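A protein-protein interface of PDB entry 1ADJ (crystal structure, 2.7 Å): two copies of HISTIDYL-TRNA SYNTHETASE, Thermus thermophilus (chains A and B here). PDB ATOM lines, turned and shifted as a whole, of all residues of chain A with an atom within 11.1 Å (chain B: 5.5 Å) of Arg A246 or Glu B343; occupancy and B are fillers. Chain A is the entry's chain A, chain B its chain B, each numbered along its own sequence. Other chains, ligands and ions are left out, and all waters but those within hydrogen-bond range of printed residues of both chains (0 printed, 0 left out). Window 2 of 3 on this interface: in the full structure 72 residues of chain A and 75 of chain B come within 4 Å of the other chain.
A ring nitrogen (ND1) of His A243 is in hydrogen-bond range of the side-chain hydroxyl (OH) of Tyr B346. The guanidinium group (NH1) of Arg A246 lies within salt-bridge range of the side-chain carboxylate (OE2) of Glu B343 (3.0 Å).
OD1 of Asn A136 lies within hydrogen-bond range of N of Ile A138, at 2.8 Å. OE1 of Glu B343 lies within salt-bridge range of NH2 of Arg B409.
CG2 of Val B341 touches CD1 of Ile A138, 3.998 Å away. Ile A138 touches Ala B342. CG2 of Ile A138 touches CG of Phe B345, at 3.7 Å. CE1 of Phe B345 touches CB of Glu A142, 3.7 Å away. NH1 of Arg A246 touches CD2 of Tyr B346, 3.1 Å away. Phe B345 touches Leu A247 (CE2 to CD1, 3.4 Å). Tyr B346 touches Leu A247 (CD1 to CD2, 3.7 Å).
Of chain B, only Glu B343 (3.0 Å) and Tyr B346 (3.1 Å) come within 4 Å of Arg A246. Printed residues of chain A within 4 Å of Glu B343: Arg A246 (3.0 Å). No residue of chain A comes within 4 Å of Glu B339. No residue of chain A comes within 4 Å of Ala B340. Ala B342 touches just one residue of chain A: Ile A138. No residue of chain A comes within 4 Å of Ala B344. No residue of chain A comes within 4 Å of Leu B347. Of the printed residues of chain B, Ile A138 touches Val B341, Ala B342 and Phe B345. Printed residues of chain B within 4 Å of Glu A142: Phe B345. Of the printed residues of chain A, Val B341 touches Ile A138. Of the printed residues of chain B, His A243 touches Tyr B346. Printed residues of chain A within 4 Å of Phe B345: Ile A138, Glu A142 and Leu A247. Glu A245 touches none of the printed residues of chain B. Ser A248 touches none of the printed residues of chain B. The nearest residue of chain B that does not touch Arg A246 is Arg B409 (4.2 Å). The nearest residue of chain A that does not touch Glu B343 is Ile A138 (6.2 Å).
Hydrophobic or aromatic side chains of chain B that line the printed part of chain A: Val B341, Phe B345 and Tyr B346. Printed residues of chain A that touch a printed residue of chain B: Ile A138, Glu A142, His A243, Arg A246 and Leu A247. Hydrophobic or aromatic side chains of chain A that line the printed part of chain B: Ile A138, His A243 and Leu A247. Among the printed residues, Asp or Glu carboxylates within 4 Å of a Lys or Arg side-chain nitrogen of the other chain: Arg A246 with Glu B343.
No position is printed for both chains. Of the 9 pairs that touch across the chains among the printed residues, none has its exchanged pair printed and touching as well.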
ATOM      1  N   ASN A 136      -8.256 -33.384   1.854  1.00  0.00           N
ATOM      2  CA  ASN A 136      -7.640 -32.574   0.807  1.00  0.00           C
ATOM      3  C   ASN A 136      -8.231 -32.744  -0.598  1.00  0.00           C
ATOM      4  O   ASN A 136      -8.262 -33.845  -1.145  1.00  0.00           O
ATOM      5  CB  ASN A 136      -6.138 -32.834   0.779  1.00  0.00           C
ATOM      6  CG  ASN A 136      -5.366 -31.726   0.106  1.00  0.00           C
ATOM      7  OD1 ASN A 136      -5.694 -31.300  -1.011  1.00  0.00           O
ATOM      8  ND2 ASN A 136      -4.327 -31.249   0.780  1.00  0.00           N
ATOM      9  N   PRO A 137      -8.695 -31.640  -1.215  1.00  0.00           N
ATOM     10  CA  PRO A 137      -9.284 -31.675  -2.560  1.00  0.00           C
ATOM     11  C   PRO A 137      -8.317 -32.092  -3.666  1.00  0.00           C
ATOM     12  O   PRO A 137      -8.736 -32.299  -4.800  1.00  0.00           O
ATOM     13  CB  PRO A 137      -9.802 -30.252  -2.747  1.00  0.00           C
ATOM     14  CG  PRO A 137      -8.867 -29.440  -1.905  1.00  0.00           C
ATOM     15  CD  PRO A 137      -8.751 -30.275  -0.660  1.00  0.00           C
ATOM     16  N   ILE A 138      -7.028 -32.201  -3.342  1.00  0.00           N
ATOM     17  CA  ILE A 138      -6.031 -32.639  -4.315  1.00  0.00           C
ATOM     18  C   ILE A 138      -6.332 -34.096  -4.671  1.00  0.00           C
ATOM     19  O   ILE A 138      -6.247 -34.494  -5.834  1.00  0.00           O
ATOM     20  CB  ILE A 138      -4.599 -32.518  -3.748  1.00  0.00           C
ATOM     21  CG1 ILE A 138      -4.111 -31.073  -3.865  1.00  0.00           C
ATOM     22  CG2 ILE A 138      -3.647 -33.444  -4.478  1.00  0.00           C
ATOM     23  CD1 ILE A 138      -2.709 -30.846  -3.323  1.00  0.00           C
ATOM     24  N   ALA A 141      -9.185 -34.375  -7.161  1.00  0.00           N
ATOM     25  CA  ALA A 141      -8.694 -34.066  -8.501  1.00  0.00           C
ATOM     26  C   ALA A 141      -7.919 -35.276  -9.018  1.00  0.00           C
ATOM     27  O   ALA A 141      -8.143 -35.725 -10.139  1.00  0.00           O
ATOM     28  CB  ALA A 141      -7.799 -32.822  -8.471  1.00  0.00           C
ATOM     29  N   GLU A 142      -7.054 -35.825  -8.171  1.00  0.00           N
ATOM     30  CA  GLU A 142      -6.239 -36.988  -8.514  1.00  0.00           C
ATOM     31  C   GLU A 142      -7.121 -38.164  -8.909  1.00  0.00           C
ATOM     32  O   GLU A 142      -6.891 -38.815  -9.930  1.00  0.00           O
ATOM     33  CB  GLU A 142      -5.361 -37.389  -7.328  1.00  0.00           C
ATOM     34  CG  GLU A 142      -4.373 -38.500  -7.622  1.00  0.00           C
ATOM     35  CD  GLU A 142      -3.454 -38.774  -6.441  1.00  0.00           C
ATOM     36  OE1 GLU A 142      -3.975 -39.053  -5.335  1.00  0.00           O
ATOM     37  OE2 GLU A 142      -2.211 -38.704  -6.610  1.00  0.00           O
ATOM     38  N   VAL A 145      -8.457 -37.551 -12.302  1.00  0.00           N
ATOM     39  CA  VAL A 145      -7.423 -37.675 -13.319  1.00  0.00           C
ATOM     40  C   VAL A 145      -7.039 -39.136 -13.532  1.00  0.00           C
ATOM     41  O   VAL A 145      -6.794 -39.558 -14.664  1.00  0.00           O
ATOM     42  CB  VAL A 145      -6.158 -36.881 -12.942  1.00  0.00           C
ATOM     43  CG1 VAL A 145      -5.178 -36.858 -14.098  1.00  0.00           C
ATOM     44  CG2 VAL A 145      -6.529 -35.477 -12.562  1.00  0.00           C
ATOM     45  N   TYR A 148      -9.716 -40.836 -15.547  1.00  0.00           N
ATOM     46  CA  TYR A 148      -9.597 -40.291 -16.894  1.00  0.00           C
ATOM     47  C   TYR A 148      -8.425 -40.938 -17.631  1.00  0.00           C
ATOM     48  O   TYR A 148      -8.564 -41.401 -18.767  1.00  0.00           O
ATOM     49  CB  TYR A 148      -9.407 -38.769 -16.808  1.00  0.00           C
ATOM     50  CG  TYR A 148      -9.337 -38.059 -18.140  1.00  0.00           C
ATOM     51  CD1 TYR A 148     -10.440 -38.028 -18.997  1.00  0.00           C
ATOM     52  CD2 TYR A 148      -8.165 -37.408 -18.545  1.00  0.00           C
ATOM     53  CE1 TYR A 148     -10.382 -37.365 -20.225  1.00  0.00           C
ATOM     54  CE2 TYR A 148      -8.094 -36.744 -19.773  1.00  0.00           C
ATOM     55  CZ  TYR A 148      -9.205 -36.726 -20.608  1.00  0.00           C
ATOM     56  OH  TYR A 148      -9.142 -36.082 -21.827  1.00  0.00           O
ATOM     57  N   LEU A 163     -18.307 -33.327 -13.697  1.00  0.00           N
ATOM     58  CA  LEU A 163     -17.998 -33.067 -12.295  1.00  0.00           C
ATOM     59  C   LEU A 163     -19.150 -32.323 -11.636  1.00  0.00           C
ATOM     60  O   LEU A 163     -19.919 -31.635 -12.308  1.00  0.00           O
ATOM     61  CB  LEU A 163     -16.719 -32.234 -12.195  1.00  0.00           C
ATOM     62  CG  LEU A 163     -16.249 -31.777 -10.814  1.00  0.00           C
ATOM     63  CD1 LEU A 163     -15.990 -32.979  -9.933  1.00  0.00           C
ATOM     64  CD2 LEU A 163     -14.989 -30.941 -10.950  1.00  0.00           C
ATOM     65  N   LEU A 237     -15.039 -27.698  -3.803  1.00  0.00           N
ATOM     66  CA  LEU A 237     -15.272 -27.990  -5.214  1.00  0.00           C
ATOM     67  C   LEU A 237     -14.457 -27.075  -6.126  1.00  0.00           C
ATOM     68  O   LEU A 237     -13.947 -27.514  -7.158  1.00  0.00           O
ATOM     69  CB  LEU A 237     -16.755 -27.875  -5.559  1.00  0.00           C
ATOM     70  CG  LEU A 237     -17.127 -28.037  -7.036  1.00  0.00           C
ATOM     71  CD1 LEU A 237     -16.737 -29.419  -7.551  1.00  0.00           C
ATOM     72  CD2 LEU A 237     -18.617 -27.809  -7.212  1.00  0.00           C
ATOM     73  N   LYS A 238     -14.316 -25.810  -5.738  1.00  0.00           N
ATOM     74  CA  LYS A 238     -13.565 -24.872  -6.550  1.00  0.00           C
ATOM     75  C   LYS A 238     -12.110 -25.306  -6.606  1.00  0.00           C
ATOM     76  O   LYS A 238     -11.470 -25.215  -7.651  1.00  0.00           O
ATOM     77  CB  LYS A 238     -13.697 -23.445  -6.005  1.00  0.00           C
ATOM     78  CG  LYS A 238     -13.526 -22.365  -7.074  1.00  0.00           C
ATOM     79  CD  LYS A 238     -14.603 -22.483  -8.170  1.00  0.00           C
ATOM     80  CE  LYS A 238     -14.333 -21.563  -9.381  1.00  0.00           C
ATOM     81  NZ  LYS A 238     -13.164 -21.976 -10.234  1.00  0.00           N
ATOM     82  N   GLU A 239     -11.604 -25.815  -5.489  1.00  0.00           N
ATOM     83  CA  GLU A 239     -10.221 -26.293  -5.410  1.00  0.00           C
ATOM     84  C   GLU A 239     -10.008 -27.421  -6.403  1.00  0.00           C
ATOM     85  O   GLU A 239      -8.977 -27.491  -7.076  1.00  0.00           O
ATOM     86  CB  GLU A 239      -9.910 -26.806  -4.005  1.00  0.00           C
ATOM     87  CG  GLU A 239      -9.671 -25.724  -2.983  1.00  0.00           C
ATOM     88  CD  GLU A 239      -8.429 -24.925  -3.301  1.00  0.00           C
ATOM     89  OE1 GLU A 239      -8.519 -24.048  -4.169  1.00  0.00           O
ATOM     90  OE2 GLU A 239      -7.360 -25.198  -2.713  1.00  0.00           O
ATOM     91  N   VAL A 240     -10.988 -28.312  -6.475  1.00  0.00           N
ATOM     92  CA  VAL A 240     -10.936 -29.446  -7.378  1.00  0.00           C
ATOM     93  C   VAL A 240     -10.900 -28.952  -8.828  1.00  0.00           C
ATOM     94  O   VAL A 240     -10.091 -29.425  -9.630  1.00  0.00           O
ATOM     95  CB  VAL A 240     -12.153 -30.396  -7.149  1.00  0.00           C
ATOM     96  CG1 VAL A 240     -12.087 -31.588  -8.090  1.00  0.00           C
ATOM     97  CG2 VAL A 240     -12.185 -30.872  -5.702  1.00  0.00           C
ATOM     98  N   GLU A 241     -11.746 -27.977  -9.154  1.00  0.00           N
ATOM     99  CA  GLU A 241     -11.786 -27.433 -10.510  1.00  0.00           C
ATOM    100  C   GLU A 241     -10.465 -26.746 -10.836  1.00  0.00           C
ATOM    101  O   GLU A 241      -9.975 -26.817 -11.959  1.00  0.00           O
ATOM    102  CB  GLU A 241     -12.928 -26.436 -10.661  1.00  0.00           C
ATOM    103  CG  GLU A 241     -14.298 -27.012 -10.413  1.00  0.00           C
ATOM    104  CD  GLU A 241     -15.417 -26.040 -10.752  1.00  0.00           C
ATOM    105  OE1 GLU A 241     -15.808 -25.986 -11.936  1.00  0.00           O
ATOM    106  OE2 GLU A 241     -15.914 -25.340  -9.840  1.00  0.00           O
ATOM    107  N   ARG A 242      -9.883 -26.091  -9.841  1.00  0.00           N
ATOM    108  CA  ARG A 242      -8.620 -25.399 -10.020  1.00  0.00           C
ATOM    109  C   ARG A 242      -7.579 -26.409 -10.480  1.00  0.00           C
ATOM    110  O   ARG A 242      -6.893 -26.190 -11.483  1.00  0.00           O
ATOM    111  CB  ARG A 242      -8.177 -24.767  -8.702  1.00  0.00           C
ATOM    112  CG  ARG A 242      -7.348 -23.531  -8.875  1.00  0.00           C
ATOM    113  CD  ARG A 242      -6.827 -23.026  -7.550  1.00  0.00           C
ATOM    114  NE  ARG A 242      -5.471 -23.485  -7.265  1.00  0.00           N
ATOM    115  CZ  ARG A 242      -5.078 -23.991  -6.100  1.00  0.00           C
ATOM    116  NH1 ARG A 242      -5.936 -24.124  -5.098  1.00  0.00           N
ATOM    117  NH2 ARG A 242      -3.808 -24.324  -5.923  1.00  0.00           N
ATOM    118  N   HIS A 243      -7.512 -27.538  -9.773  1.00  0.00           N
ATOM    119  CA  HIS A 243      -6.556 -28.606 -10.078  1.00  0.00           C
ATOM    120  C   HIS A 243      -6.783 -29.247 -11.436  1.00  0.00           C
ATOM    121  O   HIS A 243      -5.830 -29.457 -12.187  1.00  0.00           O
ATOM    122  CB  HIS A 243      -6.584 -29.687  -9.000  1.00  0.00           C
ATOM    123  CG  HIS A 243      -6.232 -29.192  -7.630  1.00  0.00           C
ATOM    124  ND1 HIS A 243      -5.267 -28.231  -7.409  1.00  0.00           N
ATOM    125  CD2 HIS A 243      -6.722 -29.520  -6.412  1.00  0.00           C
ATOM    126  CE1 HIS A 243      -5.180 -27.988  -6.112  1.00  0.00           C
ATOM    127  NE2 HIS A 243      -6.053 -28.756  -5.486  1.00  0.00           N
ATOM    128  N   LEU A 244      -8.037 -29.546 -11.763  1.00  0.00           N
ATOM    129  CA  LEU A 244      -8.354 -30.168 -13.047  1.00  0.00           C
ATOM    130  C   LEU A 244      -8.015 -29.276 -14.227  1.00  0.00           C
ATOM    131  O   LEU A 244      -7.472 -29.745 -15.230  1.00  0.00           O
ATOM    132  CB  LEU A 244      -9.818 -30.584 -13.103  1.00  0.00           C
ATOM    133  CG  LEU A 244     -10.172 -31.733 -12.162  1.00  0.00           C
ATOM    134  CD1 LEU A 244     -11.644 -32.081 -12.309  1.00  0.00           C
ATOM    135  CD2 LEU A 244      -9.292 -32.942 -12.473  1.00  0.00           C
ATOM    136  N   GLU A 245      -8.331 -27.992 -14.107  1.00  0.00           N
ATOM    137  CA  GLU A 245      -8.032 -27.022 -15.155  1.00  0.00           C
ATOM    138  C   GLU A 245      -6.513 -26.968 -15.363  1.00  0.00           C
ATOM    139  O   GLU A 245      -6.030 -27.019 -16.495  1.00  0.00           O
ATOM    140  CB  GLU A 245      -8.605 -25.645 -14.768  1.00  0.00           C
ATOM    141  CG  GLU A 245      -7.819 -24.417 -15.245  1.00  0.00           C
ATOM    142  CD  GLU A 245      -7.215 -23.635 -14.080  1.00  0.00           C
ATOM    143  OE1 GLU A 245      -7.988 -23.017 -13.307  1.00  0.00           O
ATOM    144  OE2 GLU A 245      -5.971 -23.646 -13.932  1.00  0.00           O
ATOM    145  N   ARG A 246      -5.767 -26.923 -14.261  1.00  0.00           N
ATOM    146  CA  ARG A 246      -4.313 -26.880 -14.319  1.00  0.00           C
ATOM    147  C   ARG A 246      -3.771 -28.131 -15.006  1.00  0.00           C
ATOM    148  O   ARG A 246      -2.823 -28.055 -15.791  1.00  0.00           O
ATOM    149  CB  ARG A 246      -3.726 -26.734 -12.910  1.00  0.00           C
ATOM    150  CG  ARG A 246      -2.220 -26.904 -12.833  1.00  0.00           C
ATOM    151  CD  ARG A 246      -1.471 -25.907 -13.684  1.00  0.00           C
ATOM    152  NE  ARG A 246      -0.082 -26.320 -13.848  1.00  0.00           N
ATOM    153  CZ  ARG A 246       0.890 -26.064 -12.974  1.00  0.00           C
ATOM    154  NH1 ARG A 246       0.639 -25.378 -11.864  1.00  0.00           N
ATOM    155  NH2 ARG A 246       2.113 -26.536 -13.191  1.00  0.00           N
ATOM    156  N   LEU A 247      -4.378 -29.278 -14.715  1.00  0.00           N
ATOM    157  CA  LEU A 247      -3.958 -30.536 -15.321  1.00  0.00           C
ATOM    158  C   LEU A 247      -4.564 -30.692 -16.714  1.00  0.00           C
ATOM    159  O   LEU A 247      -4.385 -31.714 -17.365  1.00  0.00           O
ATOM    160  CB  LEU A 247      -4.336 -31.726 -14.427  1.00  0.00           C
ATOM    161  CG  LEU A 247      -3.606 -31.804 -13.082  1.00  0.00           C
ATOM    162  CD1 LEU A 247      -4.248 -32.851 -12.211  1.00  0.00           C
ATOM    163  CD2 LEU A 247      -2.139 -32.093 -13.278  1.00  0.00           C
ATOM    164  N   SER A 248      -5.303 -29.681 -17.153  1.00  0.00           N
ATOM    165  CA  SER A 248      -5.928 -29.671 -18.473  1.00  0.00           C
ATOM    166  C   SER A 248      -6.903 -30.817 -18.740  1.00  0.00           C
ATOM    167  O   SER A 248      -7.017 -31.297 -19.873  1.00  0.00           O
ATOM    168  CB  SER A 248      -4.856 -29.618 -19.575  1.00  0.00           C
ATOM    169  OG  SER A 248      -4.092 -28.422 -19.500  1.00  0.00           O
ATOM    170  N   VAL A 249      -7.613 -31.252 -17.704  1.00  0.00           N
ATOM    171  CA  VAL A 249      -8.593 -32.327 -17.853  1.00  0.00           C
ATOM    172  C   VAL A 249      -9.911 -31.687 -18.288  1.00  0.00           C
ATOM    173  O   VAL A 249     -10.554 -30.987 -17.505  1.00  0.00           O
ATOM    174  CB  VAL A 249      -8.815 -33.077 -16.521  1.00  0.00           C
ATOM    175  CG1 VAL A 249      -9.770 -34.233 -16.719  1.00  0.00           C
ATOM    176  CG2 VAL A 249      -7.504 -33.573 -15.973  1.00  0.00           C
ATOM    177  N   PRO A 250     -10.314 -31.887 -19.554  1.00  0.00           N
ATOM    178  CA  PRO A 250     -11.570 -31.297 -20.039  1.00  0.00           C
ATOM    179  C   PRO A 250     -12.801 -31.873 -19.344  1.00  0.00           C
ATOM    180  O   PRO A 250     -13.076 -33.073 -19.426  1.00  0.00           O
ATOM    181  CB  PRO A 250     -11.548 -31.627 -21.532  1.00  0.00           C
ATOM    182  CG  PRO A 250     -10.799 -32.927 -21.574  1.00  0.00           C
ATOM    183  CD  PRO A 250      -9.667 -32.691 -20.605  1.00  0.00           C
ATOM    184  N   TYR A 251     -13.540 -31.023 -18.645  1.00  0.00           N
ATOM    185  CA  TYR A 251     -14.727 -31.483 -17.946  1.00  0.00           C
ATOM    186  C   TYR A 251     -15.887 -30.525 -18.129  1.00  0.00           C
ATOM    187  O   TYR A 251     -15.737 -29.436 -18.686  1.00  0.00           O
ATOM    188  CB  TYR A 251     -14.433 -31.676 -16.454  1.00  0.00           C
ATOM    189  CG  TYR A 251     -14.216 -30.398 -15.686  1.00  0.00           C
ATOM    190  CD1 TYR A 251     -12.964 -29.788 -15.644  1.00  0.00           C
ATOM    191  CD2 TYR A 251     -15.273 -29.782 -15.015  1.00  0.00           C
ATOM    192  CE1 TYR A 251     -12.771 -28.590 -14.952  1.00  0.00           C
ATOM    193  CE2 TYR A 251     -15.093 -28.586 -14.319  1.00  0.00           C
ATOM    194  CZ  TYR A 251     -13.840 -27.995 -14.294  1.00  0.00           C
ATOM    195  OH  TYR A 251     -13.658 -26.806 -13.625  1.00  0.00           O
ATOM    196  N   GLU B 339       1.837 -23.528  -1.131  1.00  0.00           N
ATOM    197  CA  GLU B 339       1.682 -23.409  -2.575  1.00  0.00           C
ATOM    198  C   GLU B 339       2.323 -24.612  -3.274  1.00  0.00           C
ATOM    199  O   GLU B 339       1.826 -25.086  -4.300  1.00  0.00           O
ATOM    200  CB  GLU B 339       2.346 -22.112  -3.049  1.00  0.00           C
ATOM    201  CG  GLU B 339       2.194 -21.798  -4.542  1.00  0.00           C
ATOM    202  CD  GLU B 339       2.992 -20.559  -4.983  1.00  0.00           C
ATOM    203  OE1 GLU B 339       3.263 -19.679  -4.133  1.00  0.00           O
ATOM    204  OE2 GLU B 339       3.318 -20.454  -6.191  1.00  0.00           O
ATOM    205  N   ALA B 340       3.409 -25.116  -2.689  1.00  0.00           N
ATOM    206  CA  ALA B 340       4.143 -26.249  -3.248  1.00  0.00           C
ATOM    207  C   ALA B 340       3.404 -27.582  -3.261  1.00  0.00           C
ATOM    208  O   ALA B 340       3.659 -28.398  -4.143  1.00  0.00           O
ATOM    209  CB  ALA B 340       5.484 -26.413  -2.550  1.00  0.00           C
ATOM    210  N   VAL B 341       2.486 -27.806  -2.319  1.00  0.00           N
ATOM    211  CA  VAL B 341       1.765 -29.080  -2.276  1.00  0.00           C
ATOM    212  C   VAL B 341       1.072 -29.380  -3.599  1.00  0.00           C
ATOM    213  O   VAL B 341       1.215 -30.473  -4.147  1.00  0.00           O
ATOM    214  CB  VAL B 341       0.751 -29.188  -1.093  1.00  0.00           C
ATOM    215  CG1 VAL B 341       1.436 -28.897   0.231  1.00  0.00           C
ATOM    216  CG2 VAL B 341      -0.424 -28.267  -1.296  1.00  0.00           C
ATOM    217  N   ALA B 342       0.380 -28.390  -4.148  1.00  0.00           N
ATOM    218  CA  ALA B 342      -0.314 -28.575  -5.414  1.00  0.00           C
ATOM    219  C   ALA B 342       0.699 -28.759  -6.536  1.00  0.00           C
ATOM    220  O   ALA B 342       0.498 -29.568  -7.438  1.00  0.00           O
ATOM    221  CB  ALA B 342      -1.217 -27.390  -5.704  1.00  0.00           C
ATOM    222  N   GLU B 343       1.790 -28.006  -6.481  1.00  0.00           N
ATOM    223  CA  GLU B 343       2.828 -28.112  -7.498  1.00  0.00           C
ATOM    224  C   GLU B 343       3.443 -29.499  -7.490  1.00  0.00           C
ATOM    225  O   GLU B 343       3.744 -30.043  -8.549  1.00  0.00           O
ATOM    226  CB  GLU B 343       3.895 -27.041  -7.301  1.00  0.00           C
ATOM    227  CG  GLU B 343       3.388 -25.631  -7.572  1.00  0.00           C
ATOM    228  CD  GLU B 343       2.838 -25.446  -8.990  1.00  0.00           C
ATOM    229  OE1 GLU B 343       3.502 -25.863  -9.964  1.00  0.00           O
ATOM    230  OE2 GLU B 343       1.738 -24.869  -9.130  1.00  0.00           O
ATOM    231  N   ALA B 344       3.587 -30.081  -6.299  1.00  0.00           N
ATOM    232  CA  ALA B 344       4.133 -31.431  -6.140  1.00  0.00           C
ATOM    233  C   ALA B 344       3.184 -32.407  -6.843  1.00  0.00           C
ATOM    234  O   ALA B 344       3.616 -33.292  -7.591  1.00  0.00           O
ATOM    235  CB  ALA B 344       4.259 -31.787  -4.666  1.00  0.00           C
ATOM    236  N   PHE B 345       1.887 -32.227  -6.613  1.00  0.00           N
ATOM    237  CA  PHE B 345       0.878 -33.059  -7.240  1.00  0.00           C
ATOM    238  C   PHE B 345       0.986 -32.957  -8.764  1.00  0.00           C
ATOM    239  O   PHE B 345       0.998 -33.976  -9.457  1.00  0.00           O
ATOM    240  CB  PHE B 345      -0.514 -32.648  -6.755  1.00  0.00           C
ATOM    241  CG  PHE B 345      -1.634 -33.203  -7.583  1.00  0.00           C
ATOM    242  CD1 PHE B 345      -1.712 -34.569  -7.853  1.00  0.00           C
ATOM    243  CD2 PHE B 345      -2.606 -32.355  -8.116  1.00  0.00           C
ATOM    244  CE1 PHE B 345      -2.746 -35.087  -8.648  1.00  0.00           C
ATOM    245  CE2 PHE B 345      -3.646 -32.860  -8.910  1.00  0.00           C
ATOM    246  CZ  PHE B 345      -3.712 -34.233  -9.177  1.00  0.00           C
ATOM    247  N   TYR B 346       1.110 -31.736  -9.283  1.00  0.00           N
ATOM    248  CA  TYR B 346       1.227 -31.533 -10.727  1.00  0.00           C
ATOM    249  C   TYR B 346       2.478 -32.206 -11.289  1.00  0.00           C
ATOM    250  O   TYR B 346       2.433 -32.845 -12.342  1.00  0.00           O
ATOM    251  CB  TYR B 346       1.282 -30.045 -11.062  1.00  0.00           C
ATOM    252  CG  TYR B 346       0.098 -29.244 -10.580  1.00  0.00           C
ATOM    253  CD1 TYR B 346      -1.183 -29.792 -10.556  1.00  0.00           C
ATOM    254  CD2 TYR B 346       0.260 -27.930 -10.143  1.00  0.00           C
ATOM    255  CE1 TYR B 346      -2.273 -29.048 -10.108  1.00  0.00           C
ATOM    256  CE2 TYR B 346      -0.819 -27.184  -9.696  1.00  0.00           C
ATOM    257  CZ  TYR B 346      -2.082 -27.749  -9.679  1.00  0.00           C
ATOM    258  OH  TYR B 346      -3.154 -27.016  -9.224  1.00  0.00           O
ATOM    259  N   LEU B 347       3.600 -32.035 -10.599  1.00  0.00           N
ATOM    260  CA  LEU B 347       4.850 -32.632 -11.031  1.00  0.00           C
ATOM    261  C   LEU B 347       4.711 -34.152 -11.022  1.00  0.00           C
ATOM    262  O   LEU B 347       5.074 -34.821 -11.990  1.00  0.00           O
ATOM    263  CB  LEU B 347       5.996 -32.195 -10.117  1.00  0.00           C
ATOM    264  CG  LEU B 347       7.371 -32.741 -10.505  1.00  0.00           C
ATOM    265  CD1 LEU B 347       7.763 -32.272 -11.907  1.00  0.00           C
ATOM    266  CD2 LEU B 347       8.403 -32.309  -9.484  1.00  0.00           C
ATOM    267  N   ALA B 348       4.155 -34.688  -9.939  1.00  0.00           N
ATOM    268  CA  ALA B 348       3.954 -36.122  -9.812  1.00  0.00           C
ATOM    269  C   ALA B 348       3.180 -36.624 -11.029  1.00  0.00           C
ATOM    270  O   ALA B 348       3.582 -37.584 -11.684  1.00  0.00           O
ATOM    271  CB  ALA B 348       3.197 -36.429  -8.539  1.00  0.00           C
ATOM    272  N   LEU B 384      10.413 -29.306  -2.874  1.00  0.00           N
ATOM    273  CA  LEU B 384       9.776 -28.207  -3.588  1.00  0.00           C
ATOM    274  C   LEU B 384       9.509 -27.053  -2.640  1.00  0.00           C
ATOM    275  O   LEU B 384       8.485 -27.019  -1.951  1.00  0.00           O
ATOM    276  CB  LEU B 384       8.470 -28.643  -4.247  1.00  0.00           C
ATOM    277  CG  LEU B 384       8.611 -29.280  -5.627  1.00  0.00           C
ATOM    278  CD1 LEU B 384       7.238 -29.585  -6.191  1.00  0.00           C
ATOM    279  CD2 LEU B 384       9.367 -28.326  -6.543  1.00  0.00           C
ATOM    280  N   LEU B 389      10.477 -23.517  -6.837  1.00  0.00           N
ATOM    281  CA  LEU B 389       9.195 -23.146  -7.435  1.00  0.00           C
ATOM    282  C   LEU B 389       9.385 -21.979  -8.391  1.00  0.00           C
ATOM    283  O   LEU B 389       8.878 -21.988  -9.517  1.00  0.00           O
ATOM    284  CB  LEU B 389       8.173 -22.757  -6.365  1.00  0.00           C
ATOM    285  CG  LEU B 389       7.433 -23.904  -5.680  1.00  0.00           C
ATOM    286  CD1 LEU B 389       6.328 -23.346  -4.788  1.00  0.00           C
ATOM    287  CD2 LEU B 389       6.842 -24.822  -6.730  1.00  0.00           C
ATOM    288  N   ARG B 409      12.585 -29.091 -14.014  1.00  0.00           N
ATOM    289  CA  ARG B 409      11.477 -30.036 -14.073  1.00  0.00           C
ATOM    290  C   ARG B 409      11.543 -31.000 -15.264  1.00  0.00           C
ATOM    291  O   ARG B 409      11.245 -32.181 -15.121  1.00  0.00           O
ATOM    292  CB  ARG B 409      10.147 -29.278 -14.101  1.00  0.00           C
ATOM    293  CG  ARG B 409       9.674 -28.748 -12.759  1.00  0.00           C
ATOM    294  CD  ARG B 409       8.377 -27.979 -12.935  1.00  0.00           C
ATOM    295  NE  ARG B 409       7.515 -28.078 -11.760  1.00  0.00           N
ATOM    296  CZ  ARG B 409       6.244 -28.477 -11.799  1.00  0.00           C
ATOM    297  NH1 ARG B 409       5.684 -28.813 -12.959  1.00  0.00           N
ATOM    298  NH2 ARG B 409       5.530 -28.560 -10.680  1.00  0.00           N
